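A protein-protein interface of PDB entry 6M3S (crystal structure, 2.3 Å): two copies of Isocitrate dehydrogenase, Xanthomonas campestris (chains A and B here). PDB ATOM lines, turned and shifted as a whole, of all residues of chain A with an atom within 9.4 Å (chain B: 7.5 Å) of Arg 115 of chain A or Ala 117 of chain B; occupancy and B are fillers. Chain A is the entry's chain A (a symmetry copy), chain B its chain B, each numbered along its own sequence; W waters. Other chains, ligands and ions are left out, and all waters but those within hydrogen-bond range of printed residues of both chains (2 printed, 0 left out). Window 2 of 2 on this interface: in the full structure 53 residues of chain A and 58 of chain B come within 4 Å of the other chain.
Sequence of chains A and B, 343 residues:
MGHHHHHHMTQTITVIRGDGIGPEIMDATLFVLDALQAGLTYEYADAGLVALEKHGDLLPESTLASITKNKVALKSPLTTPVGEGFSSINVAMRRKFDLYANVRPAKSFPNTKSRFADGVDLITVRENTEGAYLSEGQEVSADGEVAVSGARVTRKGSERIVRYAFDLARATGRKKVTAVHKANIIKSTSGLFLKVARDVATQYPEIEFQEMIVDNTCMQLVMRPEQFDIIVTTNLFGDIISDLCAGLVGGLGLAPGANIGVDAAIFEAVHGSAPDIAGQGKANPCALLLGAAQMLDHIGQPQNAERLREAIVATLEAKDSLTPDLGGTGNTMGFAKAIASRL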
ATOM      1  N   SER A 108       4.245 -14.908  28.419  1.00  0.00           N
ATOM      2  CA  SER A 108       4.546 -14.809  26.970  1.00  0.00           C
ATOM      3  C   SER A 108       4.418 -13.347  26.523  1.00  0.00           C
ATOM      4  O   SER A 108       3.393 -12.713  26.849  1.00  0.00           O
ATOM      5  CB  SER A 108       3.623 -15.691  26.165  1.00  0.00           C
ATOM      6  OG  SER A 108       4.094 -17.019  26.120  1.00  0.00           O
ATOM      7  N   PHE A 109       5.437 -12.857  25.817  1.00  0.00           N
ATOM      8  CA  PHE A 109       5.485 -11.528  25.164  1.00  0.00           C
ATOM      9  C   PHE A 109       5.575 -11.734  23.657  1.00  0.00           C
ATOM     10  O   PHE A 109       5.971 -12.803  23.189  1.00  0.00           O
ATOM     11  CB  PHE A 109       6.694 -10.710  25.641  1.00  0.00           C
ATOM     12  CG  PHE A 109       6.698 -10.402  27.116  1.00  0.00           C
ATOM     13  CD1 PHE A 109       5.803  -9.486  27.648  1.00  0.00           C
ATOM     14  CD2 PHE A 109       7.560 -11.069  27.976  1.00  0.00           C
ATOM     15  CE1 PHE A 109       5.789  -9.221  29.010  1.00  0.00           C
ATOM     16  CE2 PHE A 109       7.546 -10.798  29.333  1.00  0.00           C
ATOM     17  CZ  PHE A 109       6.664  -9.874  29.846  1.00  0.00           C
ATOM     18  N   ASN A 111       7.011 -11.203  19.693  1.00  0.00           N
ATOM     19  CA  ASN A 111       8.238 -10.994  18.871  1.00  0.00           C
ATOM     20  C   ASN A 111       9.469 -11.409  19.677  1.00  0.00           C
ATOM     21  O   ASN A 111      10.554 -10.853  19.461  1.00  0.00           O
ATOM     22  CB  ASN A 111       8.322  -9.555  18.352  1.00  0.00           C
ATOM     23  CG  ASN A 111       7.164  -9.224  17.433  1.00  0.00           C
ATOM     24  OD1 ASN A 111       6.604 -10.121  16.808  1.00  0.00           O
ATOM     25  ND2 ASN A 111       6.789  -7.956  17.347  1.00  0.00           N
ATOM     26  N   THR A 112       9.317 -12.426  20.514  1.00  0.00           N
ATOM     27  CA  THR A 112      10.195 -12.652  21.687  1.00  0.00           C
ATOM     28  C   THR A 112      11.167 -13.805  21.426  1.00  0.00           C
ATOM     29  O   THR A 112      11.854 -14.188  22.387  1.00  0.00           O
ATOM     30  CB  THR A 112       9.340 -12.847  22.945  1.00  0.00           C
ATOM     31  OG1 THR A 112      10.230 -12.973  24.054  1.00  0.00           O
ATOM     32  CG2 THR A 112       8.417 -14.046  22.865  1.00  0.00           C
ATOM     33  N   LYS A 113      11.246 -14.335  20.200  1.00  0.00           N
ATOM     34  CA  LYS A 113      12.336 -15.272  19.804  1.00  0.00           C
ATOM     35  C   LYS A 113      12.302 -16.568  20.645  1.00  0.00           C
ATOM     36  O   LYS A 113      13.305 -17.332  20.629  1.00  0.00           O
ATOM     37  CB  LYS A 113      13.685 -14.561  19.962  1.00  0.00           C
ATOM     38  CG  LYS A 113      14.852 -15.163  19.183  1.00  0.00           C
ATOM     39  CD  LYS A 113      16.164 -14.421  19.389  1.00  0.00           C
ATOM     40  CE  LYS A 113      17.365 -15.089  18.750  1.00  0.00           C
ATOM     41  NZ  LYS A 113      18.637 -14.670  19.392  1.00  0.00           N
ATOM     42  N   SER A 114      11.198 -16.839  21.357  1.00  0.00           N
ATOM     43  CA  SER A 114      11.000 -18.081  22.149  1.00  0.00           C
ATOM     44  C   SER A 114      10.574 -19.201  21.198  1.00  0.00           C
ATOM     45  O   SER A 114       9.820 -18.908  20.258  1.00  0.00           O
ATOM     46  CB  SER A 114       9.982 -17.887  23.237  1.00  0.00           C
ATOM     47  OG  SER A 114       8.719 -17.555  22.684  1.00  0.00           O
ATOM     48  N   ARG A 115      11.004 -20.438  21.468  1.00  0.00           N
ATOM     49  CA  ARG A 115      10.665 -21.645  20.655  1.00  0.00           C
ATOM     50  C   ARG A 115       9.178 -21.977  20.826  1.00  0.00           C
ATOM     51  O   ARG A 115       8.707 -22.914  20.166  1.00  0.00           O
ATOM     52  CB  ARG A 115      11.505 -22.859  21.076  1.00  0.00           C
ATOM     53  CG  ARG A 115      13.012 -22.642  21.024  1.00  0.00           C
ATOM     54  CD  ARG A 115      13.573 -22.758  19.620  1.00  0.00           C
ATOM     55  NE  ARG A 115      13.550 -24.143  19.173  1.00  0.00           N
ATOM     56  CZ  ARG A 115      14.368 -24.673  18.265  1.00  0.00           C
ATOM     57  NH1 ARG A 115      15.306 -23.931  17.689  1.00  0.00           N
ATOM     58  NH2 ARG A 115      14.256 -25.956  17.947  1.00  0.00           N
ATOM     59  N   PHE A 116       8.465 -21.229  21.675  1.00  0.00           N
ATOM     60  CA  PHE A 116       7.167 -21.651  22.252  1.00  0.00           C
ATOM     61  C   PHE A 116       6.017 -20.833  21.699  1.00  0.00           C
ATOM     62  O   PHE A 116       6.255 -19.788  21.071  1.00  0.00           O
ATOM     63  CB  PHE A 116       7.156 -21.545  23.779  1.00  0.00           C
ATOM     64  CG  PHE A 116       7.486 -22.869  24.393  1.00  0.00           C
ATOM     65  CD1 PHE A 116       8.807 -23.244  24.549  1.00  0.00           C
ATOM     66  CD2 PHE A 116       6.486 -23.787  24.652  1.00  0.00           C
ATOM     67  CE1 PHE A 116       9.123 -24.498  25.032  1.00  0.00           C
ATOM     68  CE2 PHE A 116       6.808 -25.034  25.150  1.00  0.00           C
ATOM     69  CZ  PHE A 116       8.124 -25.380  25.340  1.00  0.00           C
ATOM     70  N   ALA A 117       4.815 -21.326  22.009  1.00  0.00           N
ATOM     71  CA  ALA A 117       3.504 -20.752  21.639  1.00  0.00           C
ATOM     72  C   ALA A 117       3.386 -19.424  22.373  1.00  0.00           C
ATOM     73  O   ALA A 117       4.400 -18.972  22.933  1.00  0.00           O
ATOM     74  CB  ALA A 117       2.369 -21.684  22.011  1.00  0.00           C
ATOM     75  N   ASP A 118       2.184 -18.861  22.398  1.00  0.00           N
ATOM     76  CA  ASP A 118       1.910 -17.551  23.026  1.00  0.00           C
ATOM     77  C   ASP A 118       0.890 -17.748  24.155  1.00  0.00           C
ATOM     78  O   ASP A 118       0.105 -16.809  24.404  1.00  0.00           O
ATOM     79  CB  ASP A 118       1.464 -16.566  21.946  1.00  0.00           C
ATOM     80  CG  ASP A 118       1.707 -15.111  22.301  1.00  0.00           C
ATOM     81  OD1 ASP A 118       1.063 -14.647  23.267  1.00  0.00           O
ATOM     82  OD2 ASP A 118       2.537 -14.447  21.612  1.00  0.00           O
ATOM     83  N   VAL A 120       1.851 -19.084  27.505  1.00  0.00           N
ATOM     84  CA  VAL A 120       2.526 -19.238  28.831  1.00  0.00           C
ATOM     85  C   VAL A 120       2.108 -18.098  29.768  1.00  0.00           C
ATOM     86  O   VAL A 120       2.388 -16.915  29.461  1.00  0.00           O
ATOM     87  CB  VAL A 120       4.057 -19.290  28.700  1.00  0.00           C
ATOM     88  CG1 VAL A 120       4.701 -19.576  30.052  1.00  0.00           C
ATOM     89  CG2 VAL A 120       4.504 -20.311  27.658  1.00  0.00           C
ATOM     90  N   VAL A 222       8.052 -28.107  29.339  1.00  0.00           N
ATOM     91  CA  VAL A 222       8.543 -27.958  27.948  1.00  0.00           C
ATOM     92  C   VAL A 222       7.514 -28.544  26.983  1.00  0.00           C
ATOM     93  O   VAL A 222       7.722 -28.360  25.785  1.00  0.00           O
ATOM     94  CB  VAL A 222       9.942 -28.558  27.754  1.00  0.00           C
ATOM     95  CG1 VAL A 222      10.935 -27.960  28.733  1.00  0.00           C
ATOM     96  CG2 VAL A 222       9.924 -30.059  27.851  1.00  0.00           C
ATOM     97  N   MET A 223       6.469 -29.234  27.444  1.00  0.00           N
ATOM     98  CA  MET A 223       5.498 -29.864  26.504  1.00  0.00           C
ATOM     99  C   MET A 223       4.204 -29.055  26.484  1.00  0.00           C
ATOM    100  O   MET A 223       3.758 -28.755  25.398  1.00  0.00           O
ATOM    101  CB  MET A 223       5.182 -31.317  26.842  1.00  0.00           C
ATOM    102  CG  MET A 223       6.394 -32.183  26.761  1.00  0.00           C
ATOM    103  SD  MET A 223       6.084 -33.695  25.866  1.00  0.00           S
ATOM    104  CE  MET A 223       5.916 -33.060  24.200  1.00  0.00           C
ATOM    105  N   PRO A 225       3.291 -25.965  28.908  1.00  0.00           N
ATOM    106  CA  PRO A 225       3.371 -25.035  30.034  1.00  0.00           C
ATOM    107  C   PRO A 225       2.034 -24.350  30.338  1.00  0.00           C
ATOM    108  O   PRO A 225       1.923 -23.791  31.393  1.00  0.00           O
ATOM    109  CB  PRO A 225       4.417 -24.009  29.581  1.00  0.00           C
ATOM    110  CG  PRO A 225       4.420 -24.113  28.063  1.00  0.00           C
ATOM    111  CD  PRO A 225       4.133 -25.571  27.767  1.00  0.00           C
ATOM    112  N   GLU A 226       1.066 -24.409  29.410  1.00  0.00           N
ATOM    113  CA  GLU A 226      -0.264 -23.740  29.517  1.00  0.00           C
ATOM    114  C   GLU A 226      -1.041 -24.336  30.682  1.00  0.00           C
ATOM    115  O   GLU A 226      -1.953 -23.665  31.161  1.00  0.00           O
ATOM    116  CB  GLU A 226      -1.120 -23.918  28.250  1.00  0.00           C
ATOM    117  CG  GLU A 226      -0.487 -23.379  26.961  1.00  0.00           C
ATOM    118  CD  GLU A 226       0.399 -24.356  26.183  1.00  0.00           C
ATOM    119  OE1 GLU A 226       0.474 -25.537  26.601  1.00  0.00           O
ATOM    120  OE2 GLU A 226       1.032 -23.919  25.164  1.00  0.00           O
ATOM    121  N   ALA A 246      11.788 -18.804  32.333  1.00  0.00           N
ATOM    122  CA  ALA A 246      12.343 -17.615  31.633  1.00  0.00           C
ATOM    123  C   ALA A 246      12.619 -18.005  30.173  1.00  0.00           C
ATOM    124  O   ALA A 246      12.177 -17.312  29.262  1.00  0.00           O
ATOM    125  CB  ALA A 246      13.600 -17.131  32.302  1.00  0.00           C
ATOM    126  N   GLY A 247      13.300 -19.127  29.957  1.00  0.00           N
ATOM    127  CA  GLY A 247      13.531 -19.663  28.606  1.00  0.00           C
ATOM    128  C   GLY A 247      12.232 -19.824  27.833  1.00  0.00           C
ATOM    129  O   GLY A 247      12.248 -19.568  26.622  1.00  0.00           O
ATOM    130  N   LEU A 248      11.140 -20.222  28.496  1.00  0.00           N
ATOM    131  CA  LEU A 248       9.827 -20.475  27.837  1.00  0.00           C
ATOM    132  C   LEU A 248       9.270 -19.185  27.221  1.00  0.00           C
ATOM    133  O   LEU A 248       8.473 -19.293  26.256  1.00  0.00           O
ATOM    134  CB  LEU A 248       8.796 -21.001  28.840  1.00  0.00           C
ATOM    135  CG  LEU A 248       8.963 -22.428  29.362  1.00  0.00           C
ATOM    136  CD1 LEU A 248       7.760 -22.772  30.220  1.00  0.00           C
ATOM    137  CD2 LEU A 248       9.116 -23.429  28.232  1.00  0.00           C
ATOM    138  N   VAL A 249       9.598 -18.017  27.784  1.00  0.00           N
ATOM    139  CA  VAL A 249       8.932 -16.732  27.414  1.00  0.00           C
ATOM    140  C   VAL A 249       9.943 -15.792  26.734  1.00  0.00           C
ATOM    141  O   VAL A 249       9.698 -14.589  26.734  1.00  0.00           O
ATOM    142  CB  VAL A 249       8.263 -16.084  28.643  1.00  0.00           C
ATOM    143  CG1 VAL A 249       7.220 -17.014  29.253  1.00  0.00           C
ATOM    144  CG2 VAL A 249       9.248 -15.643  29.726  1.00  0.00           C
ATOM    145  N   GLY A 250      11.052 -16.297  26.197  1.00  0.00           N
ATOM    146  CA  GLY A 250      11.983 -15.480  25.390  1.00  0.00           C
ATOM    147  C   GLY A 250      13.366 -15.310  26.007  1.00  0.00           C
ATOM    148  O   GLY A 250      14.283 -14.852  25.299  1.00  0.00           O
ATOM    149  N   GLY A 251      13.543 -15.688  27.271  1.00  0.00           N
ATOM    150  CA  GLY A 251      14.868 -15.785  27.913  1.00  0.00           C
ATOM    151  C   GLY A 251      14.949 -14.928  29.166  1.00  0.00           C
ATOM    152  O   GLY A 251      13.932 -14.282  29.513  1.00  0.00           O
ATOM    153  N   SER B 108      15.803 -35.843  18.461  1.00  0.00           N
ATOM    154  CA  SER B 108      14.546 -35.478  17.764  1.00  0.00           C
ATOM    155  C   SER B 108      14.045 -36.682  16.960  1.00  0.00           C
ATOM    156  O   SER B 108      14.863 -37.392  16.363  1.00  0.00           O
ATOM    157  CB  SER B 108      14.713 -34.275  16.907  1.00  0.00           C
ATOM    158  OG  SER B 108      15.075 -33.136  17.682  1.00  0.00           O
ATOM    159  N   PHE B 109      12.742 -36.936  17.051  1.00  0.00           N
ATOM    160  CA  PHE B 109      11.984 -37.928  16.257  1.00  0.00           C
ATOM    161  C   PHE B 109      10.953 -37.201  15.395  1.00  0.00           C
ATOM    162  O   PHE B 109      10.478 -36.122  15.734  1.00  0.00           O
ATOM    163  CB  PHE B 109      11.289 -38.939  17.178  1.00  0.00           C
ATOM    164  CG  PHE B 109      12.205 -39.989  17.757  1.00  0.00           C
ATOM    165  CD1 PHE B 109      12.639 -41.062  16.991  1.00  0.00           C
ATOM    166  CD2 PHE B 109      12.639 -39.905  19.072  1.00  0.00           C
ATOM    167  CE1 PHE B 109      13.485 -42.026  17.524  1.00  0.00           C
ATOM    168  CE2 PHE B 109      13.481 -40.870  19.603  1.00  0.00           C
ATOM    169  CZ  PHE B 109      13.898 -41.928  18.830  1.00  0.00           C
ATOM    170  N   SER B 114       6.232 -32.571  20.235  1.00  0.00           N
ATOM    171  CA  SER B 114       7.257 -31.678  20.821  1.00  0.00           C
ATOM    172  C   SER B 114       7.227 -30.331  20.082  1.00  0.00           C
ATOM    173  O   SER B 114       6.953 -30.315  18.854  1.00  0.00           O
ATOM    174  CB  SER B 114       8.625 -32.298  20.840  1.00  0.00           C
ATOM    175  OG  SER B 114       9.569 -31.434  20.226  1.00  0.00           O
ATOM    176  N   ARG B 115       7.526 -29.251  20.812  1.00  0.00           N
ATOM    177  CA  ARG B 115       7.437 -27.837  20.360  1.00  0.00           C
ATOM    178  C   ARG B 115       8.732 -27.433  19.650  1.00  0.00           C
ATOM    179  O   ARG B 115       8.852 -26.270  19.282  1.00  0.00           O
ATOM    180  CB  ARG B 115       7.169 -26.935  21.570  1.00  0.00           C
ATOM    181  CG  ARG B 115       6.013 -27.396  22.454  1.00  0.00           C
ATOM    182  CD  ARG B 115       4.638 -27.094  21.894  1.00  0.00           C
ATOM    183  NE  ARG B 115       4.438 -25.652  21.762  1.00  0.00           N
ATOM    184  CZ  ARG B 115       4.658 -24.931  20.655  1.00  0.00           C
ATOM    185  NH1 ARG B 115       4.456 -23.628  20.678  1.00  0.00           N
ATOM    186  NH2 ARG B 115       5.079 -25.487  19.531  1.00  0.00           N
ATOM    187  N   PHE B 116       9.668 -28.365  19.485  1.00  0.00           N
ATOM    188  CA  PHE B 116      11.042 -28.119  18.986  1.00  0.00           C
ATOM    189  C   PHE B 116      11.198 -28.836  17.652  1.00  0.00           C
ATOM    190  O   PHE B 116      10.695 -29.970  17.521  1.00  0.00           O
ATOM    191  CB  PHE B 116      12.075 -28.585  20.021  1.00  0.00           C
ATOM    192  CG  PHE B 116      12.007 -27.787  21.294  1.00  0.00           C
ATOM    193  CD1 PHE B 116      10.933 -27.931  22.165  1.00  0.00           C
ATOM    194  CD2 PHE B 116      12.962 -26.818  21.572  1.00  0.00           C
ATOM    195  CE1 PHE B 116      10.835 -27.154  23.312  1.00  0.00           C
ATOM    196  CE2 PHE B 116      12.859 -26.041  22.716  1.00  0.00           C
ATOM    197  CZ  PHE B 116      11.795 -26.203  23.579  1.00  0.00           C
ATOM    198  N   ALA B 117      11.874 -28.189  16.702  1.00  0.00           N
ATOM    199  CA  ALA B 117      12.240 -28.750  15.385  1.00  0.00           C
ATOM    200  C   ALA B 117      13.282 -29.852  15.599  1.00  0.00           C
ATOM    201  O   ALA B 117      13.662 -30.076  16.760  1.00  0.00           O
ATOM    202  CB  ALA B 117      12.763 -27.650  14.492  1.00  0.00           C
ATOM    203  N   ASP B 118      13.781 -30.425  14.503  1.00  0.00           N
ATOM    204  CA  ASP B 118      14.541 -31.697  14.439  1.00  0.00           C
ATOM    205  C   ASP B 118      16.012 -31.544  14.885  1.00  0.00           C
ATOM    206  O   ASP B 118      16.789 -32.482  14.635  1.00  0.00           O
ATOM    207  CB  ASP B 118      14.468 -32.226  13.003  1.00  0.00           C
ATOM    208  CG  ASP B 118      15.105 -33.590  12.805  1.00  0.00           C
ATOM    209  OD1 ASP B 118      14.514 -34.588  13.280  1.00  0.00           O
ATOM    210  OD2 ASP B 118      16.190 -33.646  12.182  1.00  0.00           O
ATOM    211  N   GLY B 119      16.421 -30.466  15.552  1.00  0.00           N
ATOM    212  CA  GLY B 119      17.865 -30.243  15.799  1.00  0.00           C
ATOM    213  C   GLY B 119      18.410 -30.841  17.095  1.00  0.00           C
ATOM    214  O   GLY B 119      19.628 -30.649  17.352  1.00  0.00           O
ATOM    215  N   VAL B 120      17.585 -31.493  17.924  1.00  0.00           N
ATOM    216  CA  VAL B 120      18.035 -31.953  19.270  1.00  0.00           C
ATOM    217  C   VAL B 120      18.753 -33.295  19.126  1.00  0.00           C
ATOM    218  O   VAL B 120      18.140 -34.256  18.646  1.00  0.00           O
ATOM    219  CB  VAL B 120      16.897 -32.039  20.291  1.00  0.00           C
ATOM    220  CG1 VAL B 120      17.442 -32.400  21.658  1.00  0.00           C
ATOM    221  CG2 VAL B 120      16.130 -30.742  20.361  1.00  0.00           C
ATOM    222  N   GLN B 220      18.965 -22.511  28.719  1.00  0.00           N
ATOM    223  CA  GLN B 220      19.654 -22.735  27.419  1.00  0.00           C
ATOM    224  C   GLN B 220      19.009 -23.922  26.695  1.00  0.00           C
ATOM    225  O   GLN B 220      18.865 -23.854  25.448  1.00  0.00           O
ATOM    226  CB  GLN B 220      21.148 -23.017  27.597  1.00  0.00           C
ATOM    227  CG  GLN B 220      21.939 -21.876  28.233  1.00  0.00           C
ATOM    228  CD  GLN B 220      22.150 -20.665  27.349  1.00  0.00           C
ATOM    229  OE1 GLN B 220      22.129 -20.736  26.124  1.00  0.00           O
ATOM    230  NE2 GLN B 220      22.384 -19.531  27.983  1.00  0.00           N
ATOM    231  N   LEU B 221      18.665 -24.978  27.438  1.00  0.00           N
ATOM    232  CA  LEU B 221      18.039 -26.213  26.896  1.00  0.00           C
ATOM    233  C   LEU B 221      16.702 -25.855  26.223  1.00  0.00           C
ATOM    234  O   LEU B 221      16.368 -26.441  25.179  1.00  0.00           O
ATOM    235  CB  LEU B 221      17.827 -27.209  28.048  1.00  0.00           C
ATOM    236  CG  LEU B 221      18.600 -28.526  28.052  1.00  0.00           C
ATOM    237  CD1 LEU B 221      19.697 -28.611  27.009  1.00  0.00           C
ATOM    238  CD2 LEU B 221      19.140 -28.826  29.437  1.00  0.00           C
ATOM    239  N   VAL B 222      15.929 -24.935  26.775  1.00  0.00           N
ATOM    240  CA  VAL B 222      14.596 -24.628  26.177  1.00  0.00           C
ATOM    241  C   VAL B 222      14.706 -23.532  25.110  1.00  0.00           C
ATOM    242  O   VAL B 222      13.700 -23.293  24.444  1.00  0.00           O
ATOM    243  CB  VAL B 222      13.519 -24.294  27.217  1.00  0.00           C
ATOM    244  CG1 VAL B 222      13.379 -25.417  28.223  1.00  0.00           C
ATOM    245  CG2 VAL B 222      13.752 -22.976  27.907  1.00  0.00           C
ATOM    246  N   MET B 223      15.868 -22.920  24.899  1.00  0.00           N
ATOM    247  CA  MET B 223      16.000 -21.843  23.881  1.00  0.00           C
ATOM    248  C   MET B 223      16.805 -22.331  22.685  1.00  0.00           C
ATOM    249  O   MET B 223      16.361 -22.135  21.554  1.00  0.00           O
ATOM    250  CB  MET B 223      16.690 -20.613  24.464  1.00  0.00           C
ATOM    251  CG  MET B 223      15.926 -20.090  25.623  1.00  0.00           C
ATOM    252  SD  MET B 223      15.764 -18.336  25.561  1.00  0.00           S
ATOM    253  CE  MET B 223      14.861 -18.138  24.027  1.00  0.00           C
ATOM    254  N   ARG B 224      17.967 -22.926  22.938  1.00  0.00           N
ATOM    255  CA  ARG B 224      18.865 -23.446  21.874  1.00  0.00           C
ATOM    256  C   ARG B 224      19.387 -24.811  22.309  1.00  0.00           C
ATOM    257  O   ARG B 224      20.577 -24.998  22.517  1.00  0.00           O
ATOM    258  CB  ARG B 224      19.960 -22.428  21.524  1.00  0.00           C
ATOM    259  CG  ARG B 224      20.831 -21.968  22.689  1.00  0.00           C
ATOM    260  CD  ARG B 224      21.622 -20.692  22.387  1.00  0.00           C
ATOM    261  NE  ARG B 224      20.755 -19.521  22.364  1.00  0.00           N
ATOM    262  CZ  ARG B 224      20.431 -18.785  23.416  1.00  0.00           C
ATOM    263  NH1 ARG B 224      20.930 -19.046  24.609  1.00  0.00           N
ATOM    264  NH2 ARG B 224      19.598 -17.776  23.263  1.00  0.00           N
ATOM    265  N   PRO B 225      18.509 -25.834  22.427  1.00  0.00           N
ATOM    266  CA  PRO B 225      18.962 -27.172  22.786  1.00  0.00           C
ATOM    267  C   PRO B 225      19.974 -27.760  21.796  1.00  0.00           C
ATOM    268  O   PRO B 225      20.625 -28.713  22.151  1.00  0.00           O
ATOM    269  CB  PRO B 225      17.660 -27.983  22.815  1.00  0.00           C
ATOM    270  CG  PRO B 225      16.701 -27.197  21.955  1.00  0.00           C
ATOM    271  CD  PRO B 225      17.054 -25.755  22.216  1.00  0.00           C
ATOM    272  N   GLU B 226      20.088 -27.174  20.599  1.00  0.00           N
ATOM    273  CA  GLU B 226      20.985 -27.619  19.492  1.00  0.00           C
ATOM    274  C   GLU B 226      22.444 -27.441  19.890  1.00  0.00           C
ATOM    275  O   GLU B 226      23.257 -28.119  19.283  1.00  0.00           O
ATOM    276  CB  GLU B 226      20.785 -26.822  18.196  1.00  0.00           C
ATOM    277  CG  GLU B 226      19.377 -26.909  17.640  1.00  0.00           C
ATOM    278  CD  GLU B 226      18.347 -26.015  18.317  1.00  0.00           C
ATOM    279  OE1 GLU B 226      18.751 -25.076  19.062  1.00  0.00           O
ATOM    280  OE2 GLU B 226      17.135 -26.266  18.105  1.00  0.00           O
ATOM    281  N   LEU B 248      11.847 -32.136  25.266  1.00  0.00           N
ATOM    282  CA  LEU B 248      12.315 -31.492  24.016  1.00  0.00           C
ATOM    283  C   LEU B 248      12.080 -32.412  22.801  1.00  0.00           C
ATOM    284  O   LEU B 248      11.917 -31.878  21.688  1.00  0.00           O
ATOM    285  CB  LEU B 248      13.801 -31.160  24.157  1.00  0.00           C
ATOM    286  CG  LEU B 248      14.174 -30.129  25.220  1.00  0.00           C
ATOM    287  CD1 LEU B 248      15.663 -29.862  25.160  1.00  0.00           C
ATOM    288  CD2 LEU B 248      13.377 -28.841  25.047  1.00  0.00           C
ATOM    289  N   VAL B 249      12.101 -33.737  22.957  1.00  0.00           N
ATOM    290  CA  VAL B 249      12.099 -34.648  21.778  1.00  0.00           C
ATOM    291  C   VAL B 249      10.742 -35.361  21.655  1.00  0.00           C
ATOM    292  O   VAL B 249      10.622 -36.261  20.831  1.00  0.00           O
ATOM    293  CB  VAL B 249      13.268 -35.642  21.854  1.00  0.00           C
ATOM    294  CG1 VAL B 249      14.604 -34.923  21.829  1.00  0.00           C
ATOM    295  CG2 VAL B 249      13.177 -36.554  23.074  1.00  0.00           C
HETATM  296  O   HOH W   1       8.386 -30.043  23.640  1.00  0.00           O
HETATM  297  O   HOH W   2      11.971 -21.099  23.860  1.00  0.00           O
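The side-chain hydroxyl (OG) of Ser 108 of chain B sits at hydrogen-bond distance from the backbone carbonyl oxygen (O) of Ala 117 of chain B, at 3.5 Å. The backbone carbonyl oxygen (O) of Leu 248 of chain B lies within hydrogen-bond range of the side-chain hydroxyl (OG) of Ser 114 of chain B. The backbone NH of Gly 251 of chain A lies within hydrogen-bond range of the backbone carbonyl oxygen of Ala 246 of chain A (2.9 Å).
Met 223 of chain B touches Lys 113 of chain A. CG of Arg 115 of chain A touches O of Val 222 of chain B, 3.5 Å away. CG of Arg 115 of chain A touches O of Met 223 of chain B, 3.4 Å away. Phe 116 of chain A touches Phe 116 of chain B. O of Val 222 of chain A touches CG of Arg 115 of chain B, 3.9 Å away. Leu 248 of chain B touches Val 222 of chain A (N to CG2, 3.8 Å). CG of Arg 115 of chain B touches O of Met 223 of chain A, at 3.9 Å.
Of chain B, only Arg 115, Phe 116, Ala 117, Val 222, Met 223 and Glu 226 come within 4 Å of Arg 115 of chain A. Printed residues of chain B within 4 Å of Ala 117 of chain A: Arg 115 (2.7 Å). Printed residues of chain B within 4 Å of Met 223 of chain A: Ser 114 (3.9 Å) and Arg 115 (3.9 Å). Printed residues of chain B within 4 Å of Leu 248 of chain A: Val 222. Phe 116 of chain B touches just these residues of chain A: Arg 115 (3.6 Å) and Phe 116 (3.5 Å). Printed residues of chain A within 4 Å of Ala 117 of chain B: Arg 115. Printed residues of chain A within 4 Å of Val 222 of chain B: Arg 115, Val 222, Gly 247 and Leu 248. The nearest residue of chain B that does not touch Arg 115 of chain A is Pro 225 of chain B (4.9 Å).
Arg 115 of chain A touches Ala 117 of chain B, and with the chains exchanged Ala 117 of chain A touches Arg 115 of chain B. Positions printed for both chains: 108, 109, 114, 115, 116, 117, 118, 120, 222, 223, 225, 226, 248 and 249. Of the 20 pairs that touch across the chains among the printed residues, 13 have their exchanged pair printed and touching as well.
Hydrophobic or aromatic side chains of chain B within 4 Å of the printed part of chain A: Phe 116, Val 222 and Met 223. Of the 21 printed residues of chain A, 10 touch a printed residue of chain B. Printed residues of chain A that touch a printed residue of chain B: Lys 113, Arg 115, Phe 116, Ala 117, Val 222, Met 223, Gly 247, Leu 248, Gly 250 and Gly 251. Among the printed residues, 20 pairs touch across the chains. Among the printed residues, Asp or Glu carboxylates within 4 Å of a Lys or Arg side-chain nitrogen of the other chain: Arg 115 of chain A with Glu 226 of chain B.
Water W2 lies within hydrogen-bond range of N of Arg 115 of chain A, O of Val 222 of chain B and O of Gly 247 of chain A. Water W1 bridges O of Val 222 of chain A (2.8 Å) and N of Arg 115 of chain B (3.1 Å).
NH1 of Arg 115 of chain B sits close to N of Ala 117 of chain A (2.7 Å). OE2 of Glu 226 of chain B is in salt-bridge range of NH2 of Arg 115 of chain A, 2.9 Å away. O of Arg 115 of chain A sits close to O of Arg 115 of chain B, at 3.5 Å. N of Ala 117 of chain B lies close to NH2 of Arg 115 of chain A. SD of Met 223 of chain B lies close to O of Gly 250 of chain A (3.8 Å).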
